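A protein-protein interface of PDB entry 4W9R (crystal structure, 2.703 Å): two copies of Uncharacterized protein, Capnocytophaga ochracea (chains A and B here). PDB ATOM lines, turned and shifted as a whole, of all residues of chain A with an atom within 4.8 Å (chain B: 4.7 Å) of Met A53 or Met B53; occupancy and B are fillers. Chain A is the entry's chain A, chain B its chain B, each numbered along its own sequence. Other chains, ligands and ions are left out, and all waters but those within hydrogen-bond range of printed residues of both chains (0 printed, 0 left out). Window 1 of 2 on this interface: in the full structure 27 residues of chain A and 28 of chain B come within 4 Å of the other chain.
OG of Ser B52 sits at hydrogen-bond distance from OG of Ser A52 (3.0 Å).
O of Pro A49 sits at hydrogen-bond distance from OG of Ser A52 (2.8 Å). O of Ala A226 sits at hydrogen-bond distance from OH of Tyr A57. The backbone carbonyl oxygen of Pro B49 is in hydrogen-bond range of the side-chain hydroxyl of Ser B52 (3.0 Å). O of Ala B226 sits at hydrogen-bond distance from OH of Tyr B57 (2.8 Å).
Ser B52 touches Pro A49 (OG to CA, 3.9 Å). Tyr B56 touches Pro A49 (CD1 to CG, 3.9 Å). CE of Met B53 touches CE of Met A53 (3.6 Å). Tyr A56 touches Pro B49. Leu B222 touches Tyr A56 (CG to CE2, 3.5 Å). Met B53 touches Leu A222. Leu A222 touches Tyr B56 (CG to CE2, 3.5 Å). Tyr B57 touches Leu A222 (OH to CD1, 3.6 Å). Leu A222 touches Ala B226 (CB to CB, 3.96 Å). CB of Ala A226 touches CB of Leu B222, 3.98 Å away.
Met A53 touches just these residues of chain B: Met B53 (3.6 Å) and Leu B222 (3.8 Å). Of chain A, only Met A53 (3.6 Å) and Leu A222 (3.8 Å) come within 4 Å of Met B53. Printed residues of chain A within 4 Å of Tyr B57: Leu A222. Of the printed residues of chain B, Leu A222 touches Met B53, Tyr B56, Tyr B57 and Ala B226. Printed residues of chain B within 4 Å of Pro A49: Ser B52 (3.9 Å) and Tyr B56 (3.9 Å). Of the printed residues of chain A, Tyr B56 touches Pro A49 (3.9 Å) and Leu A222 (3.5 Å). Leu A229 touches none of the printed residues of chain B. The nearest printed residue of chain A that does not touch Met B53 is Pro A49 (5.4 Å). The nearest printed residue of chain B that does not touch Leu A222 is Ser B52 (6.2 Å).
Of the 13 printed residues of chain B, 7 touch a printed residue of chain A. Printed residues of chain B that touch a printed residue of chain A: Pro B49, Ser B52, Met B53, Tyr B56, Tyr B57, Leu B222 and Ala B226. Hydrophobic or aromatic side chains of chain B within 4 Å of the printed part of chain A: Pro B49, Met B53, Tyr B56, Tyr B57, Leu B222 and Ala B226. Among the printed residues, no Asp or Glu carboxylate lies within 4 Å of a Lys or Arg side-chain nitrogen of the other chain.
Pro A49 touches Ser B52, but with the chains exchanged Ser A52 does not touch Pro B49 (4.04 Å). Ser B52 touches its own counterpart, Ser A52. Tyr A56 touches Leu B222, and with the chains exchanged Leu A222 touches Tyr B56. Tyr A57 touches Leu B222, and with the chains exchanged Leu A222 touches Tyr B57. Positions printed for both chains: 49, 50, 51, 52, 53, 54, 55, 56, 57, 222, 225, 226 and 229. Of the 13 pairs that touch across the chains among the printed residues, 12 have their exchanged pair printed and touching as well.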
ATOM      1  N   PRO A  49       8.047   5.211 -20.114  1.00  0.00           N
ATOM      2  CA  PRO A  49       7.688   5.667 -18.764  1.00  0.00           C
ATOM      3  C   PRO A  49       6.198   5.963 -18.601  1.00  0.00           C
ATOM      4  O   PRO A  49       5.627   5.614 -17.571  1.00  0.00           O
ATOM      5  CB  PRO A  49       8.513   6.946 -18.596  1.00  0.00           C
ATOM      6  CG  PRO A  49       9.681   6.749 -19.487  1.00  0.00           C
ATOM      7  CD  PRO A  49       9.139   6.026 -20.681  1.00  0.00           C
ATOM      8  N   VAL A  50       5.583   6.589 -19.600  1.00  0.00           N
ATOM      9  CA  VAL A  50       4.160   6.911 -19.529  1.00  0.00           C
ATOM     10  C   VAL A  50       3.312   5.644 -19.445  1.00  0.00           C
ATOM     11  O   VAL A  50       2.417   5.541 -18.603  1.00  0.00           O
ATOM     12  CB  VAL A  50       3.709   7.754 -20.743  1.00  0.00           C
ATOM     13  CG1 VAL A  50       2.193   7.735 -20.882  1.00  0.00           C
ATOM     14  CG2 VAL A  50       4.214   9.182 -20.612  1.00  0.00           C
ATOM     15  N   VAL A  51       3.608   4.677 -20.307  1.00  0.00           N
ATOM     16  CA  VAL A  51       2.857   3.426 -20.339  1.00  0.00           C
ATOM     17  C   VAL A  51       3.032   2.642 -19.038  1.00  0.00           C
ATOM     18  O   VAL A  51       2.073   2.083 -18.505  1.00  0.00           O
ATOM     19  CB  VAL A  51       3.282   2.551 -21.539  1.00  0.00           C
ATOM     20  CG1 VAL A  51       2.644   1.170 -21.456  1.00  0.00           C
ATOM     21  CG2 VAL A  51       2.908   3.233 -22.845  1.00  0.00           C
ATOM     22  N   SER A  52       4.254   2.614 -18.519  1.00  0.00           N
ATOM     23  CA  SER A  52       4.527   1.876 -17.293  1.00  0.00           C
ATOM     24  C   SER A  52       3.819   2.503 -16.091  1.00  0.00           C
ATOM     25  O   SER A  52       3.394   1.797 -15.178  1.00  0.00           O
ATOM     26  CB  SER A  52       6.034   1.799 -17.034  1.00  0.00           C
ATOM     27  OG  SER A  52       6.570   3.082 -16.767  1.00  0.00           O
ATOM     28  N   MET A  53       3.698   3.827 -16.093  1.00  0.00           N
ATOM     29  CA  MET A  53       3.082   4.523 -14.969  1.00  0.00           C
ATOM     30  C   MET A  53       1.550   4.480 -14.995  1.00  0.00           C
ATOM     31  O   MET A  53       0.918   4.479 -13.937  1.00  0.00           O
ATOM     32  CB  MET A  53       3.576   5.970 -14.910  1.00  0.00           C
ATOM     33  CG  MET A  53       5.052   6.081 -14.550  1.00  0.00           C
ATOM     34  SD  MET A  53       5.642   7.891 -14.125  1.00  0.00           S
ATOM     35  CE  MET A  53       7.303   7.913 -15.148  1.00  0.00           C
ATOM     36  N   VAL A  54       0.946   4.440 -16.181  1.00  0.00           N
ATOM     37  CA  VAL A  54      -0.509   4.304 -16.251  1.00  0.00           C
ATOM     38  C   VAL A  54      -0.905   2.869 -15.904  1.00  0.00           C
ATOM     39  O   VAL A  54      -1.988   2.629 -15.374  1.00  0.00           O
ATOM     40  CB  VAL A  54      -1.087   4.696 -17.638  1.00  0.00           C
ATOM     41  CG1 VAL A  54      -0.810   6.163 -17.939  1.00  0.00           C
ATOM     42  CG2 VAL A  54      -0.544   3.806 -18.738  1.00  0.00           C
ATOM     43  N   ARG A  55      -0.019   1.922 -16.200  1.00  0.00           N
ATOM     44  CA  ARG A  55      -0.193   0.542 -15.763  1.00  0.00           C
ATOM     45  C   ARG A  55      -0.118   0.477 -14.246  1.00  0.00           C
ATOM     46  O   ARG A  55      -0.968  -0.122 -13.586  1.00  0.00           O
ATOM     47  CB  ARG A  55       0.875  -0.363 -16.381  1.00  0.00           C
ATOM     48  CG  ARG A  55       0.369  -1.288 -17.468  1.00  0.00           C
ATOM     49  CD  ARG A  55       1.504  -2.105 -18.067  1.00  0.00           C
ATOM     50  NE  ARG A  55       1.026  -3.053 -19.066  1.00  0.00           N
ATOM     51  CZ  ARG A  55       0.705  -4.315 -18.803  1.00  0.00           C
ATOM     52  NH1 ARG A  55       0.817  -4.787 -17.568  1.00  0.00           N
ATOM     53  NH2 ARG A  55       0.274  -5.108 -19.775  1.00  0.00           N
ATOM     54  N   TYR A  56       0.924   1.106 -13.714  1.00  0.00           N
ATOM     55  CA  TYR A  56       1.165   1.203 -12.282  1.00  0.00           C
ATOM     56  C   TYR A  56      -0.053   1.750 -11.546  1.00  0.00           C
ATOM     57  O   TYR A  56      -0.555   1.130 -10.608  1.00  0.00           O
ATOM     58  CB  TYR A  56       2.392   2.088 -12.044  1.00  0.00           C
ATOM     59  CG  TYR A  56       2.726   2.410 -10.605  1.00  0.00           C
ATOM     60  CD1 TYR A  56       3.508   1.554  -9.844  1.00  0.00           C
ATOM     61  CD2 TYR A  56       2.300   3.598 -10.027  1.00  0.00           C
ATOM     62  CE1 TYR A  56       3.833   1.860  -8.535  1.00  0.00           C
ATOM     63  CE2 TYR A  56       2.618   3.911  -8.721  1.00  0.00           C
ATOM     64  CZ  TYR A  56       3.386   3.041  -7.981  1.00  0.00           C
ATOM     65  OH  TYR A  56       3.704   3.354  -6.680  1.00  0.00           O
ATOM     66  N   TYR A  57      -0.535   2.904 -11.991  1.00  0.00           N
ATOM     67  CA  TYR A  57      -1.675   3.557 -11.360  1.00  0.00           C
ATOM     68  C   TYR A  57      -2.960   2.742 -11.491  1.00  0.00           C
ATOM     69  O   TYR A  57      -3.805   2.752 -10.593  1.00  0.00           O
ATOM     70  CB  TYR A  57      -1.875   4.951 -11.955  1.00  0.00           C
ATOM     71  CG  TYR A  57      -0.926   5.993 -11.402  1.00  0.00           C
ATOM     72  CD1 TYR A  57      -0.661   6.065 -10.040  1.00  0.00           C
ATOM     73  CD2 TYR A  57      -0.295   6.900 -12.240  1.00  0.00           C
ATOM     74  CE1 TYR A  57       0.200   7.014  -9.529  1.00  0.00           C
ATOM     75  CE2 TYR A  57       0.571   7.855 -11.738  1.00  0.00           C
ATOM     76  CZ  TYR A  57       0.814   7.907 -10.381  1.00  0.00           C
ATOM     77  OH  TYR A  57       1.674   8.853  -9.874  1.00  0.00           O
ATOM     78  N   LEU A 222      10.402  12.850 -15.413  1.00  0.00           N
ATOM     79  CA  LEU A 222       9.815  11.611 -14.912  1.00  0.00           C
ATOM     80  C   LEU A 222       8.848  11.896 -13.773  1.00  0.00           C
ATOM     81  O   LEU A 222       7.737  11.366 -13.737  1.00  0.00           O
ATOM     82  CB  LEU A 222      10.900  10.645 -14.436  1.00  0.00           C
ATOM     83  CG  LEU A 222      11.745   9.961 -15.507  1.00  0.00           C
ATOM     84  CD1 LEU A 222      12.731   9.000 -14.863  1.00  0.00           C
ATOM     85  CD2 LEU A 222      10.858   9.239 -16.509  1.00  0.00           C
ATOM     86  N   ILE A 225       5.563  13.510 -15.021  1.00  0.00           N
ATOM     87  CA  ILE A 225       4.576  12.552 -15.498  1.00  0.00           C
ATOM     88  C   ILE A 225       3.820  11.919 -14.334  1.00  0.00           C
ATOM     89  O   ILE A 225       2.594  11.818 -14.360  1.00  0.00           O
ATOM     90  CB  ILE A 225       5.226  11.442 -16.340  1.00  0.00           C
ATOM     91  CG1 ILE A 225       5.968  12.047 -17.532  1.00  0.00           C
ATOM     92  CG2 ILE A 225       4.177  10.451 -16.817  1.00  0.00           C
ATOM     93  CD1 ILE A 225       6.653  11.023 -18.412  1.00  0.00           C
ATOM     94  N   ALA A 226       4.564  11.498 -13.316  1.00  0.00           N
ATOM     95  CA  ALA A 226       3.978  10.855 -12.148  1.00  0.00           C
ATOM     96  C   ALA A 226       2.969  11.769 -11.459  1.00  0.00           C
ATOM     97  O   ALA A 226       1.886  11.331 -11.070  1.00  0.00           O
ATOM     98  CB  ALA A 226       5.067  10.436 -11.173  1.00  0.00           C
ATOM     99  N   LEU A 229      -0.284  12.597 -13.943  1.00  0.00           N
ATOM    100  CA  LEU A 229      -1.240  11.495 -13.945  1.00  0.00           C
ATOM    101  C   LEU A 229      -1.961  11.374 -12.609  1.00  0.00           C
ATOM    102  O   LEU A 229      -3.160  11.098 -12.561  1.00  0.00           O
ATOM    103  CB  LEU A 229      -0.536  10.179 -14.274  1.00  0.00           C
ATOM    104  CG  LEU A 229       0.059  10.080 -15.680  1.00  0.00           C
ATOM    105  CD1 LEU A 229       0.802   8.765 -15.856  1.00  0.00           C
ATOM    106  CD2 LEU A 229      -1.031  10.230 -16.732  1.00  0.00           C
ATOM    107  N   PRO B  49       7.992   0.097 -13.764  1.00  0.00           N
ATOM    108  CA  PRO B  49       8.495   1.467 -13.609  1.00  0.00           C
ATOM    109  C   PRO B  49      10.016   1.546 -13.462  1.00  0.00           C
ATOM    110  O   PRO B  49      10.624   2.456 -14.021  1.00  0.00           O
ATOM    111  CB  PRO B  49       7.803   1.950 -12.332  1.00  0.00           C
ATOM    112  CG  PRO B  49       6.539   1.179 -12.294  1.00  0.00           C
ATOM    113  CD  PRO B  49       6.898  -0.184 -12.815  1.00  0.00           C
ATOM    114  N   VAL B  50      10.617   0.611 -12.731  1.00  0.00           N
ATOM    115  CA  VAL B  50      12.069   0.592 -12.570  1.00  0.00           C
ATOM    116  C   VAL B  50      12.767   0.336 -13.905  1.00  0.00           C
ATOM    117  O   VAL B  50      13.694   1.056 -14.279  1.00  0.00           O
ATOM    118  CB  VAL B  50      12.517  -0.472 -11.547  1.00  0.00           C
ATOM    119  CG1 VAL B  50      14.027  -0.682 -11.614  1.00  0.00           C
ATOM    120  CG2 VAL B  50      12.099  -0.069 -10.142  1.00  0.00           C
ATOM    121  N   VAL B  51      12.311  -0.686 -14.623  1.00  0.00           N
ATOM    122  CA  VAL B  51      12.897  -1.038 -15.911  1.00  0.00           C
ATOM    123  C   VAL B  51      12.766   0.103 -16.920  1.00  0.00           C
ATOM    124  O   VAL B  51      13.715   0.420 -17.633  1.00  0.00           O
ATOM    125  CB  VAL B  51      12.251  -2.312 -16.494  1.00  0.00           C
ATOM    126  CG1 VAL B  51      12.738  -2.562 -17.913  1.00  0.00           C
ATOM    127  CG2 VAL B  51      12.557  -3.508 -15.610  1.00  0.00           C
ATOM    128  N   SER B  52      11.597   0.731 -16.970  1.00  0.00           N
ATOM    129  CA  SER B  52      11.372   1.809 -17.927  1.00  0.00           C
ATOM    130  C   SER B  52      12.241   3.027 -17.619  1.00  0.00           C
ATOM    131  O   SER B  52      12.688   3.722 -18.531  1.00  0.00           O
ATOM    132  CB  SER B  52       9.897   2.213 -17.952  1.00  0.00           C
ATOM    133  OG  SER B  52       9.518   2.828 -16.734  1.00  0.00           O
ATOM    134  N   MET B  53      12.480   3.285 -16.336  1.00  0.00           N
ATOM    135  CA  MET B  53      13.252   4.459 -15.942  1.00  0.00           C
ATOM    136  C   MET B  53      14.763   4.264 -16.100  1.00  0.00           C
ATOM    137  O   MET B  53      15.484   5.229 -16.347  1.00  0.00           O
ATOM    138  CB  MET B  53      12.917   4.861 -14.502  1.00  0.00           C
ATOM    139  CG  MET B  53      11.515   5.454 -14.345  1.00  0.00           C
ATOM    140  SD  MET B  53      11.123   6.141 -12.557  1.00  0.00           S
ATOM    141  CE  MET B  53       9.174   6.149 -12.640  1.00  0.00           C
ATOM    142  N   VAL B  54      15.250   3.031 -15.974  1.00  0.00           N
ATOM    143  CA  VAL B  54      16.681   2.795 -16.172  1.00  0.00           C
ATOM    144  C   VAL B  54      17.010   2.805 -17.664  1.00  0.00           C
ATOM    145  O   VAL B  54      18.127   3.142 -18.056  1.00  0.00           O
ATOM    146  CB  VAL B  54      17.164   1.463 -15.535  1.00  0.00           C
ATOM    147  CG1 VAL B  54      16.929   1.474 -14.029  1.00  0.00           C
ATOM    148  CG2 VAL B  54      16.490   0.265 -16.178  1.00  0.00           C
ATOM    149  N   ARG B  55      16.033   2.450 -18.493  1.00  0.00           N
ATOM    150  CA  ARG B  55      16.187   2.552 -19.940  1.00  0.00           C
ATOM    151  C   ARG B  55      16.136   4.013 -20.360  1.00  0.00           C
ATOM    152  O   ARG B  55      16.864   4.447 -21.252  1.00  0.00           O
ATOM    153  CB  ARG B  55      15.100   1.756 -20.662  1.00  0.00           C
ATOM    154  CG  ARG B  55      15.201   0.257 -20.474  1.00  0.00           C
ATOM    155  CD  ARG B  55      14.020  -0.462 -21.109  1.00  0.00           C
ATOM    156  NE  ARG B  55      13.843  -0.092 -22.510  1.00  0.00           N
ATOM    157  CZ  ARG B  55      14.471  -0.680 -23.523  1.00  0.00           C
ATOM    158  NH1 ARG B  55      15.322  -1.670 -23.294  1.00  0.00           N
ATOM    159  NH2 ARG B  55      14.247  -0.277 -24.766  1.00  0.00           N
ATOM    160  N   TYR B  56      15.260   4.761 -19.699  1.00  0.00           N
ATOM    161  CA  TYR B  56      15.103   6.192 -19.921  1.00  0.00           C
ATOM    162  C   TYR B  56      16.413   6.931 -19.664  1.00  0.00           C
ATOM    163  O   TYR B  56      16.906   7.659 -20.524  1.00  0.00           O
ATOM    164  CB  TYR B  56      13.986   6.723 -19.021  1.00  0.00           C
ATOM    165  CG  TYR B  56      13.801   8.224 -18.999  1.00  0.00           C
ATOM    166  CD1 TYR B  56      12.976   8.857 -19.921  1.00  0.00           C
ATOM    167  CD2 TYR B  56      14.416   9.003 -18.028  1.00  0.00           C
ATOM    168  CE1 TYR B  56      12.790  10.226 -19.889  1.00  0.00           C
ATOM    169  CE2 TYR B  56      14.239  10.371 -17.990  1.00  0.00           C
ATOM    170  CZ  TYR B  56      13.424  10.976 -18.920  1.00  0.00           C
ATOM    171  OH  TYR B  56      13.248  12.338 -18.878  1.00  0.00           O
ATOM    172  N   TYR B  57      16.976   6.729 -18.477  1.00  0.00           N
ATOM    173  CA  TYR B  57      18.234   7.362 -18.101  1.00  0.00           C
ATOM    174  C   TYR B  57      19.392   6.913 -18.986  1.00  0.00           C
ATOM    175  O   TYR B  57      20.313   7.683 -19.254  1.00  0.00           O
ATOM    176  CB  TYR B  57      18.556   7.070 -16.635  1.00  0.00           C
ATOM    177  CG  TYR B  57      17.748   7.889 -15.655  1.00  0.00           C
ATOM    178  CD1 TYR B  57      17.531   9.244 -15.868  1.00  0.00           C
ATOM    179  CD2 TYR B  57      17.201   7.308 -14.518  1.00  0.00           C
ATOM    180  CE1 TYR B  57      16.795  10.000 -14.974  1.00  0.00           C
ATOM    181  CE2 TYR B  57      16.462   8.056 -13.617  1.00  0.00           C
ATOM    182  CZ  TYR B  57      16.263   9.401 -13.851  1.00  0.00           C
ATOM    183  OH  TYR B  57      15.530  10.152 -12.961  1.00  0.00           O
ATOM    184  N   LEU B 222       6.863   6.461  -7.193  1.00  0.00           N
ATOM    185  CA  LEU B 222       7.359   6.637  -8.554  1.00  0.00           C
ATOM    186  C   LEU B 222       8.439   7.707  -8.591  1.00  0.00           C
ATOM    187  O   LEU B 222       9.488   7.524  -9.209  1.00  0.00           O
ATOM    188  CB  LEU B 222       6.227   7.013  -9.510  1.00  0.00           C
ATOM    189  CG  LEU B 222       5.196   5.940  -9.849  1.00  0.00           C
ATOM    190  CD1 LEU B 222       4.198   6.475 -10.863  1.00  0.00           C
ATOM    191  CD2 LEU B 222       5.864   4.673 -10.363  1.00  0.00           C
ATOM    192  N   ILE B 225      11.785   6.488  -7.077  1.00  0.00           N
ATOM    193  CA  ILE B 225      12.629   5.729  -7.992  1.00  0.00           C
ATOM    194  C   ILE B 225      13.406   6.661  -8.911  1.00  0.00           C
ATOM    195  O   ILE B 225      14.606   6.486  -9.120  1.00  0.00           O
ATOM    196  CB  ILE B 225      11.802   4.754  -8.849  1.00  0.00           C
ATOM    197  CG1 ILE B 225      11.029   3.785  -7.956  1.00  0.00           C
ATOM    198  CG2 ILE B 225      12.698   3.991  -9.812  1.00  0.00           C
ATOM    199  CD1 ILE B 225      10.117   2.851  -8.715  1.00  0.00           C
ATOM    200  N   ALA B 226      12.711   7.658  -9.452  1.00  0.00           N
ATOM    201  CA  ALA B 226      13.321   8.618 -10.365  1.00  0.00           C
ATOM    202  C   ALA B 226      14.465   9.372  -9.696  1.00  0.00           C
ATOM    203  O   ALA B 226      15.542   9.522 -10.271  1.00  0.00           O
ATOM    204  CB  ALA B 226      12.275   9.591 -10.880  1.00  0.00           C
ATOM    205  N   LEU B 229      17.578   6.789  -8.591  1.00  0.00           N
ATOM    206  CA  LEU B 229      18.406   6.431  -9.738  1.00  0.00           C
ATOM    207  C   LEU B 229      19.222   7.620 -10.231  1.00  0.00           C
ATOM    208  O   LEU B 229      20.373   7.468 -10.639  1.00  0.00           O
ATOM    209  CB  LEU B 229      17.541   5.891 -10.877  1.00  0.00           C
ATOM    210  CG  LEU B 229      16.819   4.569 -10.627  1.00  0.00           C
ATOM    211  CD1 LEU B 229      15.909   4.245 -11.796  1.00  0.00           C
ATOM    212  CD2 LEU B 229      17.821   3.449 -10.390  1.00  0.00           C
